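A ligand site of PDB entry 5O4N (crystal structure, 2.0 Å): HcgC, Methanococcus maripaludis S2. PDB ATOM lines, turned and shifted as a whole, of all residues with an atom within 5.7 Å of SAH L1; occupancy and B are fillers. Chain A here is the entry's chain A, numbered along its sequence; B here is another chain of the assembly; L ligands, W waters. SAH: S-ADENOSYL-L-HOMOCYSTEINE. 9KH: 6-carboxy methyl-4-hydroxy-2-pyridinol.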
ATOM      1  N   LYS A  29       7.379 -29.977  -5.473  1.00  0.00           N
ATOM      2  CA  LYS A  29       8.151 -30.675  -6.508  1.00  0.00           C
ATOM      3  C   LYS A  29       8.378 -32.125  -6.099  1.00  0.00           C
ATOM      4  O   LYS A  29       8.245 -33.020  -6.930  1.00  0.00           O
ATOM      5  CB  LYS A  29       9.488 -29.978  -6.788  1.00  0.00           C
ATOM      6  CG  LYS A  29       9.363 -28.647  -7.449  1.00  0.00           C
ATOM      7  CD  LYS A  29      10.710 -28.077  -7.804  1.00  0.00           C
ATOM      8  CE  LYS A  29      10.586 -26.756  -8.514  1.00  0.00           C
ATOM      9  NZ  LYS A  29      11.878 -26.212  -8.926  1.00  0.00           N
ATOM     10  N   PHE A  48      20.618 -35.607 -10.173  1.00  0.00           N
ATOM     11  CA  PHE A  48      21.598 -34.613 -10.614  1.00  0.00           C
ATOM     12  C   PHE A  48      21.137 -33.208 -10.204  1.00  0.00           C
ATOM     13  O   PHE A  48      20.044 -32.807 -10.582  1.00  0.00           O
ATOM     14  CB  PHE A  48      21.766 -34.643 -12.126  1.00  0.00           C
ATOM     15  CG  PHE A  48      22.573 -35.823 -12.595  1.00  0.00           C
ATOM     16  CD1 PHE A  48      21.961 -37.025 -12.875  1.00  0.00           C
ATOM     17  CD2 PHE A  48      23.940 -35.713 -12.745  1.00  0.00           C
ATOM     18  CE1 PHE A  48      22.717 -38.118 -13.307  1.00  0.00           C
ATOM     19  CE2 PHE A  48      24.689 -36.799 -13.186  1.00  0.00           C
ATOM     20  CZ  PHE A  48      24.078 -37.997 -13.454  1.00  0.00           C
ATOM     21  N   GLY A  49      21.967 -32.493  -9.442  1.00  0.00           N
ATOM     22  CA  GLY A  49      21.646 -31.135  -8.988  1.00  0.00           C
ATOM     23  C   GLY A  49      21.100 -31.103  -7.581  1.00  0.00           C
ATOM     24  O   GLY A  49      19.933 -31.422  -7.344  1.00  0.00           O
ATOM     25  N   ALA A  50      21.954 -30.738  -6.632  1.00  0.00           N
ATOM     26  CA  ALA A  50      21.617 -30.672  -5.220  1.00  0.00           C
ATOM     27  C   ALA A  50      20.835 -29.409  -4.865  1.00  0.00           C
ATOM     28  O   ALA A  50      19.937 -29.457  -4.016  1.00  0.00           O
ATOM     29  CB  ALA A  50      22.891 -30.723  -4.393  1.00  0.00           C
ATOM     30  N   TYR A  51      21.192 -28.271  -5.481  1.00  0.00           N
ATOM     31  CA  TYR A  51      20.526 -27.002  -5.221  1.00  0.00           C
ATOM     32  C   TYR A  51      19.375 -26.805  -6.224  1.00  0.00           C
ATOM     33  O   TYR A  51      19.577 -27.069  -7.396  1.00  0.00           O
ATOM     34  CB  TYR A  51      21.541 -25.849  -5.284  1.00  0.00           C
ATOM     35  CG  TYR A  51      20.968 -24.464  -5.331  1.00  0.00           C
ATOM     36  CD1 TYR A  51      20.482 -23.931  -6.530  1.00  0.00           C
ATOM     37  CD2 TYR A  51      20.957 -23.651  -4.211  1.00  0.00           C
ATOM     38  CE1 TYR A  51      19.963 -22.647  -6.586  1.00  0.00           C
ATOM     39  CE2 TYR A  51      20.440 -22.359  -4.263  1.00  0.00           C
ATOM     40  CZ  TYR A  51      19.966 -21.852  -5.460  1.00  0.00           C
ATOM     41  OH  TYR A  51      19.458 -20.582  -5.565  1.00  0.00           O
ATOM     42  N   LEU A  52      18.183 -26.323  -5.810  1.00  0.00           N
ATOM     43  CA  LEU A  52      17.755 -25.982  -4.443  1.00  0.00           C
ATOM     44  C   LEU A  52      16.743 -27.031  -3.944  1.00  0.00           C
ATOM     45  O   LEU A  52      16.670 -27.301  -2.753  1.00  0.00           O
ATOM     46  CB  LEU A  52      17.206 -24.561  -4.391  1.00  0.00           C
ATOM     47  CG  LEU A  52      16.746 -24.014  -3.030  1.00  0.00           C
ATOM     48  CD1 LEU A  52      17.796 -24.202  -1.922  1.00  0.00           C
ATOM     49  CD2 LEU A  52      16.365 -22.507  -3.170  1.00  0.00           C
ATOM     50  N   SER A  53      15.981 -27.638  -4.866  1.00  0.00           N
ATOM     51  CA  SER A  53      14.982 -28.665  -4.556  1.00  0.00           C
ATOM     52  C   SER A  53      15.584 -30.096  -4.523  1.00  0.00           C
ATOM     53  O   SER A  53      14.951 -30.983  -3.970  1.00  0.00           O
ATOM     54  CB  SER A  53      13.853 -28.611  -5.583  1.00  0.00           C
ATOM     55  OG  SER A  53      14.348 -28.915  -6.875  1.00  0.00           O
ATOM     56  N   GLY A  54      16.751 -30.298  -5.121  1.00  0.00           N
ATOM     57  CA  GLY A  54      17.383 -31.613  -5.153  1.00  0.00           C
ATOM     58  C   GLY A  54      17.606 -32.284  -3.815  1.00  0.00           C
ATOM     59  O   GLY A  54      17.429 -33.495  -3.703  1.00  0.00           O
ATOM     60  N   VAL A  71      24.248 -36.132  -7.273  1.00  0.00           N
ATOM     61  CA  VAL A  71      25.394 -35.803  -8.078  1.00  0.00           C
ATOM     62  C   VAL A  71      25.358 -34.295  -8.308  1.00  0.00           C
ATOM     63  O   VAL A  71      24.336 -33.772  -8.718  1.00  0.00           O
ATOM     64  CB  VAL A  71      25.443 -36.589  -9.411  1.00  0.00           C
ATOM     65  CG1 VAL A  71      26.642 -36.136 -10.262  1.00  0.00           C
ATOM     66  CG2 VAL A  71      25.512 -38.087  -9.147  1.00  0.00           C
ATOM     67  N   ASP A  72      26.468 -33.595  -8.036  1.00  0.00           N
ATOM     68  CA  ASP A  72      26.554 -32.166  -8.263  1.00  0.00           C
ATOM     69  C   ASP A  72      27.979 -31.823  -8.733  1.00  0.00           C
ATOM     70  O   ASP A  72      28.978 -32.356  -8.221  1.00  0.00           O
ATOM     71  CB  ASP A  72      26.150 -31.312  -7.067  1.00  0.00           C
ATOM     72  CG  ASP A  72      25.626 -29.954  -7.526  1.00  0.00           C
ATOM     73  OD1 ASP A  72      26.399 -29.224  -8.184  1.00  0.00           O
ATOM     74  OD2 ASP A  72      24.435 -29.663  -7.284  1.00  0.00           O
ATOM     75  N   ILE A  73      28.058 -30.910  -9.697  1.00  0.00           N
ATOM     76  CA  ILE A  73      29.319 -30.448 -10.275  1.00  0.00           C
ATOM     77  C   ILE A  73      30.133 -29.662  -9.207  1.00  0.00           C
ATOM     78  O   ILE A  73      31.363 -29.581  -9.322  1.00  0.00           O
ATOM     79  CB  ILE A  73      29.039 -29.609 -11.574  1.00  0.00           C
ATOM     80  CG1 ILE A  73      30.328 -29.446 -12.420  1.00  0.00           C
ATOM     81  CG2 ILE A  73      28.409 -28.239 -11.261  1.00  0.00           C
ATOM     82  CD1 ILE A  73      30.072 -29.094 -13.881  1.00  0.00           C
ATOM     83  N   GLN A  74      29.448 -29.100  -8.201  1.00  0.00           N
ATOM     84  CA  GLN A  74      30.050 -28.343  -7.104  1.00  0.00           C
ATOM     85  C   GLN A  74      30.209 -29.243  -5.825  1.00  0.00           C
ATOM     86  O   GLN A  74      29.211 -29.540  -5.162  1.00  0.00           O
ATOM     87  CB  GLN A  74      29.164 -27.146  -6.745  1.00  0.00           C
ATOM     88  CG  GLN A  74      28.874 -26.189  -7.884  1.00  0.00           C
ATOM     89  CD  GLN A  74      29.968 -25.180  -8.137  1.00  0.00           C
ATOM     90  OE1 GLN A  74      31.073 -25.250  -7.600  1.00  0.00           O
ATOM     91  NE2 GLN A  74      29.648 -24.205  -8.996  1.00  0.00           N
ATOM     92  N   LEU A  77      28.403 -28.450  -2.284  1.00  0.00           N
ATOM     93  CA  LEU A  77      26.974 -28.657  -2.134  1.00  0.00           C
ATOM     94  C   LEU A  77      26.656 -29.921  -1.330  1.00  0.00           C
ATOM     95  O   LEU A  77      25.477 -30.170  -1.065  1.00  0.00           O
ATOM     96  CB  LEU A  77      26.223 -28.621  -3.463  1.00  0.00           C
ATOM     97  CG  LEU A  77      26.137 -27.217  -4.084  1.00  0.00           C
ATOM     98  CD1 LEU A  77      25.469 -27.289  -5.421  1.00  0.00           C
ATOM     99  CD2 LEU A  77      25.356 -26.238  -3.174  1.00  0.00           C
ATOM    100  N   LEU A  91      30.671 -34.660  -9.752  1.00  0.00           N
ATOM    101  CA  LEU A  91      30.521 -35.051 -11.157  1.00  0.00           C
ATOM    102  C   LEU A  91      31.778 -35.793 -11.658  1.00  0.00           C
ATOM    103  O   LEU A  91      31.651 -36.749 -12.415  1.00  0.00           O
ATOM    104  CB  LEU A  91      30.157 -33.852 -12.051  1.00  0.00           C
ATOM    105  CG  LEU A  91      29.858 -34.133 -13.530  1.00  0.00           C
ATOM    106  CD1 LEU A  91      28.650 -35.016 -13.682  1.00  0.00           C
ATOM    107  CD2 LEU A  91      29.665 -32.848 -14.293  1.00  0.00           C
ATOM    108  N   LEU A 112      17.744 -32.540 -12.333  1.00  0.00           N
ATOM    109  CA  LEU A 112      17.201 -31.254 -11.870  1.00  0.00           C
ATOM    110  C   LEU A 112      18.145 -30.087 -12.155  1.00  0.00           C
ATOM    111  O   LEU A 112      17.950 -29.008 -11.595  1.00  0.00           O
ATOM    112  CB  LEU A 112      16.989 -31.331 -10.348  1.00  0.00           C
ATOM    113  CG  LEU A 112      16.227 -32.516  -9.820  1.00  0.00           C
ATOM    114  CD1 LEU A 112      16.306 -32.575  -8.325  1.00  0.00           C
ATOM    115  CD2 LEU A 112      14.787 -32.493 -10.295  1.00  0.00           C
ATOM    116  N   THR A 113      19.141 -30.274 -13.018  1.00  0.00           N
ATOM    117  CA  THR A 113      20.124 -29.223 -13.299  1.00  0.00           C
ATOM    118  C   THR A 113      19.601 -28.045 -14.137  1.00  0.00           C
ATOM    119  O   THR A 113      20.101 -26.932 -13.965  1.00  0.00           O
ATOM    120  CB  THR A 113      21.384 -29.813 -13.901  1.00  0.00           C
ATOM    121  OG1 THR A 113      21.070 -30.389 -15.168  1.00  0.00           O
ATOM    122  CG2 THR A 113      22.028 -30.839 -12.970  1.00  0.00           C
ATOM    123  N   GLY A 114      18.649 -28.299 -15.026  1.00  0.00           N
ATOM    124  CA  GLY A 114      18.088 -27.250 -15.862  1.00  0.00           C
ATOM    125  C   GLY A 114      19.063 -26.558 -16.803  1.00  0.00           C
ATOM    126  O   GLY A 114      19.904 -27.217 -17.416  1.00  0.00           O
ATOM    127  N   GLY A 116      21.932 -24.921 -18.727  1.00  0.00           N
ATOM    128  CA  GLY A 116      23.362 -25.160 -18.760  1.00  0.00           C
ATOM    129  C   GLY A 116      23.833 -26.336 -17.922  1.00  0.00           C
ATOM    130  O   GLY A 116      25.011 -26.436 -17.594  1.00  0.00           O
ATOM    131  N   GLY A 117      22.897 -27.214 -17.576  1.00  0.00           N
ATOM    132  CA  GLY A 117      23.119 -28.385 -16.757  1.00  0.00           C
ATOM    133  C   GLY A 117      23.731 -29.606 -17.410  1.00  0.00           C
ATOM    134  O   GLY A 117      24.586 -29.460 -18.270  1.00  0.00           O
ATOM    135  N   VAL A 118      23.289 -30.806 -16.995  1.00  0.00           N
ATOM    136  CA  VAL A 118      23.829 -32.055 -17.531  1.00  0.00           C
ATOM    137  C   VAL A 118      23.558 -32.204 -18.992  1.00  0.00           C
ATOM    138  O   VAL A 118      22.506 -31.809 -19.497  1.00  0.00           O
ATOM    139  CB  VAL A 118      23.461 -33.366 -16.792  1.00  0.00           C
ATOM    140  CG1 VAL A 118      23.768 -33.270 -15.336  1.00  0.00           C
ATOM    141  CG2 VAL A 118      22.020 -33.759 -17.026  1.00  0.00           C
ATOM    142  N   SER A 119      24.510 -32.791 -19.671  1.00  0.00           N
ATOM    143  CA  SER A 119      24.390 -32.985 -21.095  1.00  0.00           C
ATOM    144  C   SER A 119      23.583 -34.222 -21.412  1.00  0.00           C
ATOM    145  O   SER A 119      23.626 -35.204 -20.650  1.00  0.00           O
ATOM    146  CB  SER A 119      25.785 -33.162 -21.699  1.00  0.00           C
ATOM    147  OG  SER A 119      26.361 -34.391 -21.272  1.00  0.00           O
ATOM    148  N   LEU A 122      25.687 -37.500 -21.206  1.00  0.00           N
ATOM    149  CA  LEU A 122      25.880 -38.176 -19.911  1.00  0.00           C
ATOM    150  C   LEU A 122      24.620 -38.989 -19.598  1.00  0.00           C
ATOM    151  O   LEU A 122      24.727 -40.141 -19.175  1.00  0.00           O
ATOM    152  CB  LEU A 122      26.168 -37.169 -18.785  1.00  0.00           C
ATOM    153  CG  LEU A 122      26.342 -37.768 -17.360  1.00  0.00           C
ATOM    154  CD1 LEU A 122      27.493 -38.762 -17.294  1.00  0.00           C
ATOM    155  CD2 LEU A 122      26.567 -36.659 -16.360  1.00  0.00           C
ATOM    156  N   GLU A 134      13.771 -32.269 -15.186  1.00  0.00           N
ATOM    157  CA  GLU A 134      13.055 -31.053 -14.792  1.00  0.00           C
ATOM    158  C   GLU A 134      13.156 -30.047 -15.912  1.00  0.00           C
ATOM    159  O   GLU A 134      14.250 -29.761 -16.392  1.00  0.00           O
ATOM    160  CB  GLU A 134      13.610 -30.465 -13.490  1.00  0.00           C
ATOM    161  CG  GLU A 134      12.859 -29.210 -13.042  1.00  0.00           C
ATOM    162  CD  GLU A 134      13.118 -28.736 -11.632  1.00  0.00           C
ATOM    163  OE1 GLU A 134      14.177 -29.086 -11.060  1.00  0.00           O
ATOM    164  OE2 GLU A 134      12.278 -27.962 -11.113  1.00  0.00           O
ATOM    165  N   SER A 175      10.810 -22.311 -13.796  1.00  0.00           N
ATOM    166  CA  SER A 175      10.218 -23.213 -12.817  1.00  0.00           C
ATOM    167  C   SER A 175      11.168 -23.365 -11.638  1.00  0.00           C
ATOM    168  O   SER A 175      10.871 -24.104 -10.701  1.00  0.00           O
ATOM    169  CB  SER A 175      10.009 -24.577 -13.446  1.00  0.00           C
ATOM    170  OG  SER A 175      11.263 -25.047 -13.941  1.00  0.00           O
ATOM    171  N   GLY A 176      12.308 -22.693 -11.672  1.00  0.00           N
ATOM    172  CA  GLY A 176      13.297 -22.751 -10.610  1.00  0.00           C
ATOM    173  C   GLY A 176      12.731 -22.322  -9.280  1.00  0.00           C
ATOM    174  O   GLY A 176      11.965 -21.368  -9.211  1.00  0.00           O
ATOM    175  N   THR A 177      13.092 -23.035  -8.231  1.00  0.00           N
ATOM    176  CA  THR A 177      12.677 -22.791  -6.858  1.00  0.00           C
ATOM    177  C   THR A 177      12.952 -21.321  -6.480  1.00  0.00           C
ATOM    178  O   THR A 177      12.052 -20.646  -5.984  1.00  0.00           O
ATOM    179  CB  THR A 177      13.425 -23.713  -5.915  1.00  0.00           C
ATOM    180  OG1 THR A 177      13.183 -25.044  -6.314  1.00  0.00           O
ATOM    181  CG2 THR A 177      12.981 -23.571  -4.460  1.00  0.00           C
ATOM    182  N   MET A 178      14.163 -20.852  -6.720  1.00  0.00           N
ATOM    183  CA  MET A 178      14.556 -19.471  -6.432  1.00  0.00           C
ATOM    184  C   MET A 178      13.689 -18.472  -7.190  1.00  0.00           C
ATOM    185  O   MET A 178      13.230 -17.485  -6.584  1.00  0.00           O
ATOM    186  CB  MET A 178      16.045 -19.256  -6.766  1.00  0.00           C
ATOM    187  CG  MET A 178      16.589 -17.850  -6.445  1.00  0.00           C
ATOM    188  SD  MET A 178      16.363 -17.326  -4.720  1.00  0.00           S
ATOM    189  CE  MET A 178      17.258 -18.611  -3.835  1.00  0.00           C
ATOM    190  N   PHE A 213      26.827 -20.248  -4.513  1.00  0.00           N
ATOM    191  CA  PHE A 213      27.795 -20.524  -5.599  1.00  0.00           C
ATOM    192  C   PHE A 213      29.030 -19.630  -5.715  1.00  0.00           C
ATOM    193  O   PHE A 213      30.018 -20.100  -6.280  1.00  0.00           O
ATOM    194  CB  PHE A 213      27.023 -20.485  -6.921  1.00  0.00           C
ATOM    195  CG  PHE A 213      26.040 -21.627  -6.946  1.00  0.00           C
ATOM    196  CD1 PHE A 213      24.724 -21.453  -6.538  1.00  0.00           C
ATOM    197  CD2 PHE A 213      26.434 -22.899  -7.335  1.00  0.00           C
ATOM    198  CE1 PHE A 213      23.833 -22.519  -6.509  1.00  0.00           C
ATOM    199  CE2 PHE A 213      25.537 -23.954  -7.325  1.00  0.00           C
ATOM    200  CZ  PHE A 213      24.237 -23.762  -6.917  1.00  0.00           C
ATOM    201  N   ILE B   5      25.082 -19.870 -11.634  1.00  0.00           N
ATOM    202  CA  ILE B   5      25.328 -21.270 -11.266  1.00  0.00           C
ATOM    203  C   ILE B   5      26.294 -21.937 -12.256  1.00  0.00           C
ATOM    204  O   ILE B   5      27.132 -22.760 -11.861  1.00  0.00           O
ATOM    205  CB  ILE B   5      23.967 -22.008 -11.099  1.00  0.00           C
ATOM    206  CG1 ILE B   5      23.213 -21.379  -9.912  1.00  0.00           C
ATOM    207  CG2 ILE B   5      24.161 -23.485 -10.875  1.00  0.00           C
ATOM    208  CD1 ILE B   5      21.695 -21.622  -9.830  1.00  0.00           C
ATOM    209  N   THR B   6      26.179 -21.587 -13.531  1.00  0.00           N
ATOM    210  CA  THR B   6      27.023 -22.097 -14.613  1.00  0.00           C
ATOM    211  C   THR B   6      27.302 -20.921 -15.519  1.00  0.00           C
ATOM    212  O   THR B   6      26.742 -19.836 -15.315  1.00  0.00           O
ATOM    213  CB  THR B   6      26.330 -23.242 -15.432  1.00  0.00           C
ATOM    214  OG1 THR B   6      25.312 -22.694 -16.264  1.00  0.00           O
ATOM    215  CG2 THR B   6      25.807 -24.363 -14.555  1.00  0.00           C
HETATM  216  N   SAH L   1      16.134 -27.089 -10.704  1.00  0.00           N
HETATM  217  CA  SAH L   1      16.737 -26.410  -9.518  1.00  0.00           C
HETATM  218  CB  SAH L   1      17.724 -25.316  -9.936  1.00  0.00           C
HETATM  219  CG  SAH L   1      18.834 -25.861 -10.829  1.00  0.00           C
HETATM  220  SD  SAH L   1      20.391 -25.140 -10.438  1.00  0.00           S
HETATM  221  C   SAH L   1      15.673 -25.791  -8.660  1.00  0.00           C
HETATM  222  O   SAH L   1      14.566 -25.505  -9.148  1.00  0.00           O
HETATM  223  OXT SAH L   1      15.917 -25.569  -7.474  1.00  0.00           O
HETATM  224  C5' SAH L   1      21.591 -26.278 -11.058  1.00  0.00           C
HETATM  225  C4' SAH L   1      22.095 -27.235  -9.961  1.00  0.00           C
HETATM  226  O4' SAH L   1      22.709 -28.373 -10.599  1.00  0.00           O
HETATM  227  C3' SAH L   1      23.219 -26.599  -9.124  1.00  0.00           C
HETATM  228  O3' SAH L   1      23.296 -27.288  -7.860  1.00  0.00           O
HETATM  229  C2' SAH L   1      24.466 -26.886  -9.963  1.00  0.00           C
HETATM  230  O2' SAH L   1      25.697 -26.826  -9.220  1.00  0.00           O
HETATM  231  C1' SAH L   1      24.143 -28.311 -10.478  1.00  0.00           C
HETATM  232  N9  SAH L   1      24.738 -28.641 -11.792  1.00  0.00           N
HETATM  233  C8  SAH L   1      24.906 -27.813 -12.863  1.00  0.00           C
HETATM  234  N7  SAH L   1      25.463 -28.492 -13.892  1.00  0.00           N
HETATM  235  C5  SAH L   1      25.631 -29.761 -13.496  1.00  0.00           C
HETATM  236  C6  SAH L   1      26.163 -31.017 -14.081  1.00  0.00           C
HETATM  237  N6  SAH L   1      26.637 -31.039 -15.355  1.00  0.00           N
HETATM  238  N1  SAH L   1      26.154 -32.137 -13.313  1.00  0.00           N
HETATM  239  C2  SAH L   1      25.687 -32.160 -12.046  1.00  0.00           C
HETATM  240  N3  SAH L   1      25.195 -31.051 -11.461  1.00  0.00           N
HETATM  241  C4  SAH L   1      25.154 -29.853 -12.105  1.00  0.00           C
HETATM  242  C2  9KH L   2      18.113 -23.086 -13.898  1.00  0.00           C
HETATM  243  C3  9KH L   2      17.164 -22.263 -13.282  1.00  0.00           C
HETATM  244  C4  9KH L   2      17.630 -21.071 -12.693  1.00  0.00           C
HETATM  245  C6  9KH L   2      19.857 -21.559 -13.337  1.00  0.00           C
HETATM  246  O1  9KH L   2      17.739 -24.254 -14.489  1.00  0.00           O
HETATM  247  N5  9KH L   2      18.953 -20.764 -12.734  1.00  0.00           N
HETATM  248  C7  9KH L   2      19.455 -22.747 -13.921  1.00  0.00           C
HETATM  249  O8  9KH L   2      21.162 -21.198 -13.336  1.00  0.00           O
HETATM  250  C9  9KH L   2      15.699 -22.663 -13.257  1.00  0.00           C
HETATM  251  C10 9KH L   2      16.739 -20.101 -11.989  1.00  0.00           C
HETATM  252  C12 9KH L   2      16.591 -20.578 -10.549  1.00  0.00           C
HETATM  253  O13 9KH L   2      17.487 -21.261  -9.980  1.00  0.00           O
HETATM  254  O14 9KH L   2      15.526 -20.230  -9.998  1.00  0.00           O
HETATM  255  O   HOH W   1      27.501 -25.272 -10.882  1.00  0.00           O
HETATM  256  O   HOH W   2      27.247 -33.157 -17.856  1.00  0.00           O
HETATM  257  O   HOH W   3      13.530 -25.803 -12.411  1.00  0.00           O
HETATM  258  O   HOH W   4      26.985 -27.601 -16.173  1.00  0.00           O
HETATM  259  O   HOH W   5      22.688 -25.736 -14.219  1.00  0.00           O
HETATM  260  O   HOH W   6      16.506 -22.387  -7.738  1.00  0.00           O
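OD2 of Asp 72 sits at hydrogen-bond distance from O3' of SAH L1, at 2.7 Å.
The side-chain amino group (NZ) of Lys 29 is in salt-bridge range of an oxygen (O) of SAH L1 (2.8 Å).
The backbone carbonyl oxygen (O) of Leu 112 lies within hydrogen-bond range of a nitrogen (N) of SAH L1.
OE1 of Glu 134 is in salt-bridge range of N of SAH L1.
The backbone NH of Leu 52 is in hydrogen-bond range of an oxygen (OXT) of SAH L1, 2.9 Å away.
N of Thr 177 is in hydrogen-bond range of O of SAH L1, at 3.0 Å.
OG1 of Thr 177 sits at hydrogen-bond distance from OXT of SAH L1 (3.0 Å).
The backbone NH (N) of Tyr 51 sits at hydrogen-bond distance from an oxygen (O3') of SAH L1 (3.3 Å).
N of Ser 53 sits at hydrogen-bond distance from OXT of SAH L1.
The backbone NH of Ile 73 sits at hydrogen-bond distance from a nitrogen (N3) of SAH L1 (3.4 Å).
OD1 of Asp 72 lies within hydrogen-bond range of N of Gln 74.
O of Asp 72 is in hydrogen-bond range of N of Leu 91 (3.2 Å).
N of Ala 50 lies within hydrogen-bond range of OD2 of Asp 72.
The side-chain amino group (NZ) of Lys 29 lies within hydrogen-bond range of the side-chain hydroxyl (OG1) of Thr 177, at 3.1 Å.
The side-chain amino group (NZ) of Lys 29 sits at hydrogen-bond distance from the backbone carbonyl oxygen (O) of Ser 175.
O of Phe 48 sits at hydrogen-bond distance from N of Leu 112 (2.9 Å).
The backbone NH of Val 118 sits at hydrogen-bond distance from the side-chain hydroxyl of Thr 113.
N of Gly 49 is in hydrogen-bond range of O of Val 71 (2.8 Å).
Residues that only touch SAH L1: Gly 49 (3.4 Å), Ala 50 (3.9 Å), Val 71 (3.9 Å), Gln 74 (3.5 Å), Leu 77 (3.3 Å), Leu 91 (3.7 Å), Thr 113 (3.3 Å), Gly 117 (3.7 Å), Val 118 (3.3 Å), Gly 176 (3.4 Å), Phe 213 (3.4 Å), Ile 5 of chain B (3.5 Å) and Thr 6 of chain B (3.9 Å).
Hydrophobic or aromatic side chains that line SAH L1: Tyr 51, Leu 52, Ile 73, Leu 77, Leu 91, Val 118, Phe 213 and Ile 5 of chain B.
Of the 30 residues printed, 22 come within 4 Å of SAH L1.
Water W4 bridges O of Gly 116 and N7 of SAH L1.
Water W1 lies within hydrogen-bond range of the backbone carbonyl oxygen of Ile 5 of chain B (2.7 Å), an oxygen (O2') of SAH L1 (2.9 Å) and the side-chain amide nitrogen of Gln 74 (3.1 Å).
Water W6 lies within hydrogen-bond range of O13 of 9KH L2 (2.7 Å), N of Met 178 (3.0 Å) and OXT of SAH L1 (3.2 Å).
Water W2 bridges the backbone NH of Ser 119 (3.3 Å) and a nitrogen (N6) of SAH L1 (3.3 Å).
Water W3 lies within hydrogen-bond range of the side-chain carboxylate (OE2) of Glu 134, the side-chain hydroxyl (OG) of Ser 175, a nitrogen (N) of SAH L1 and the backbone NH (N) of Gly 176.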
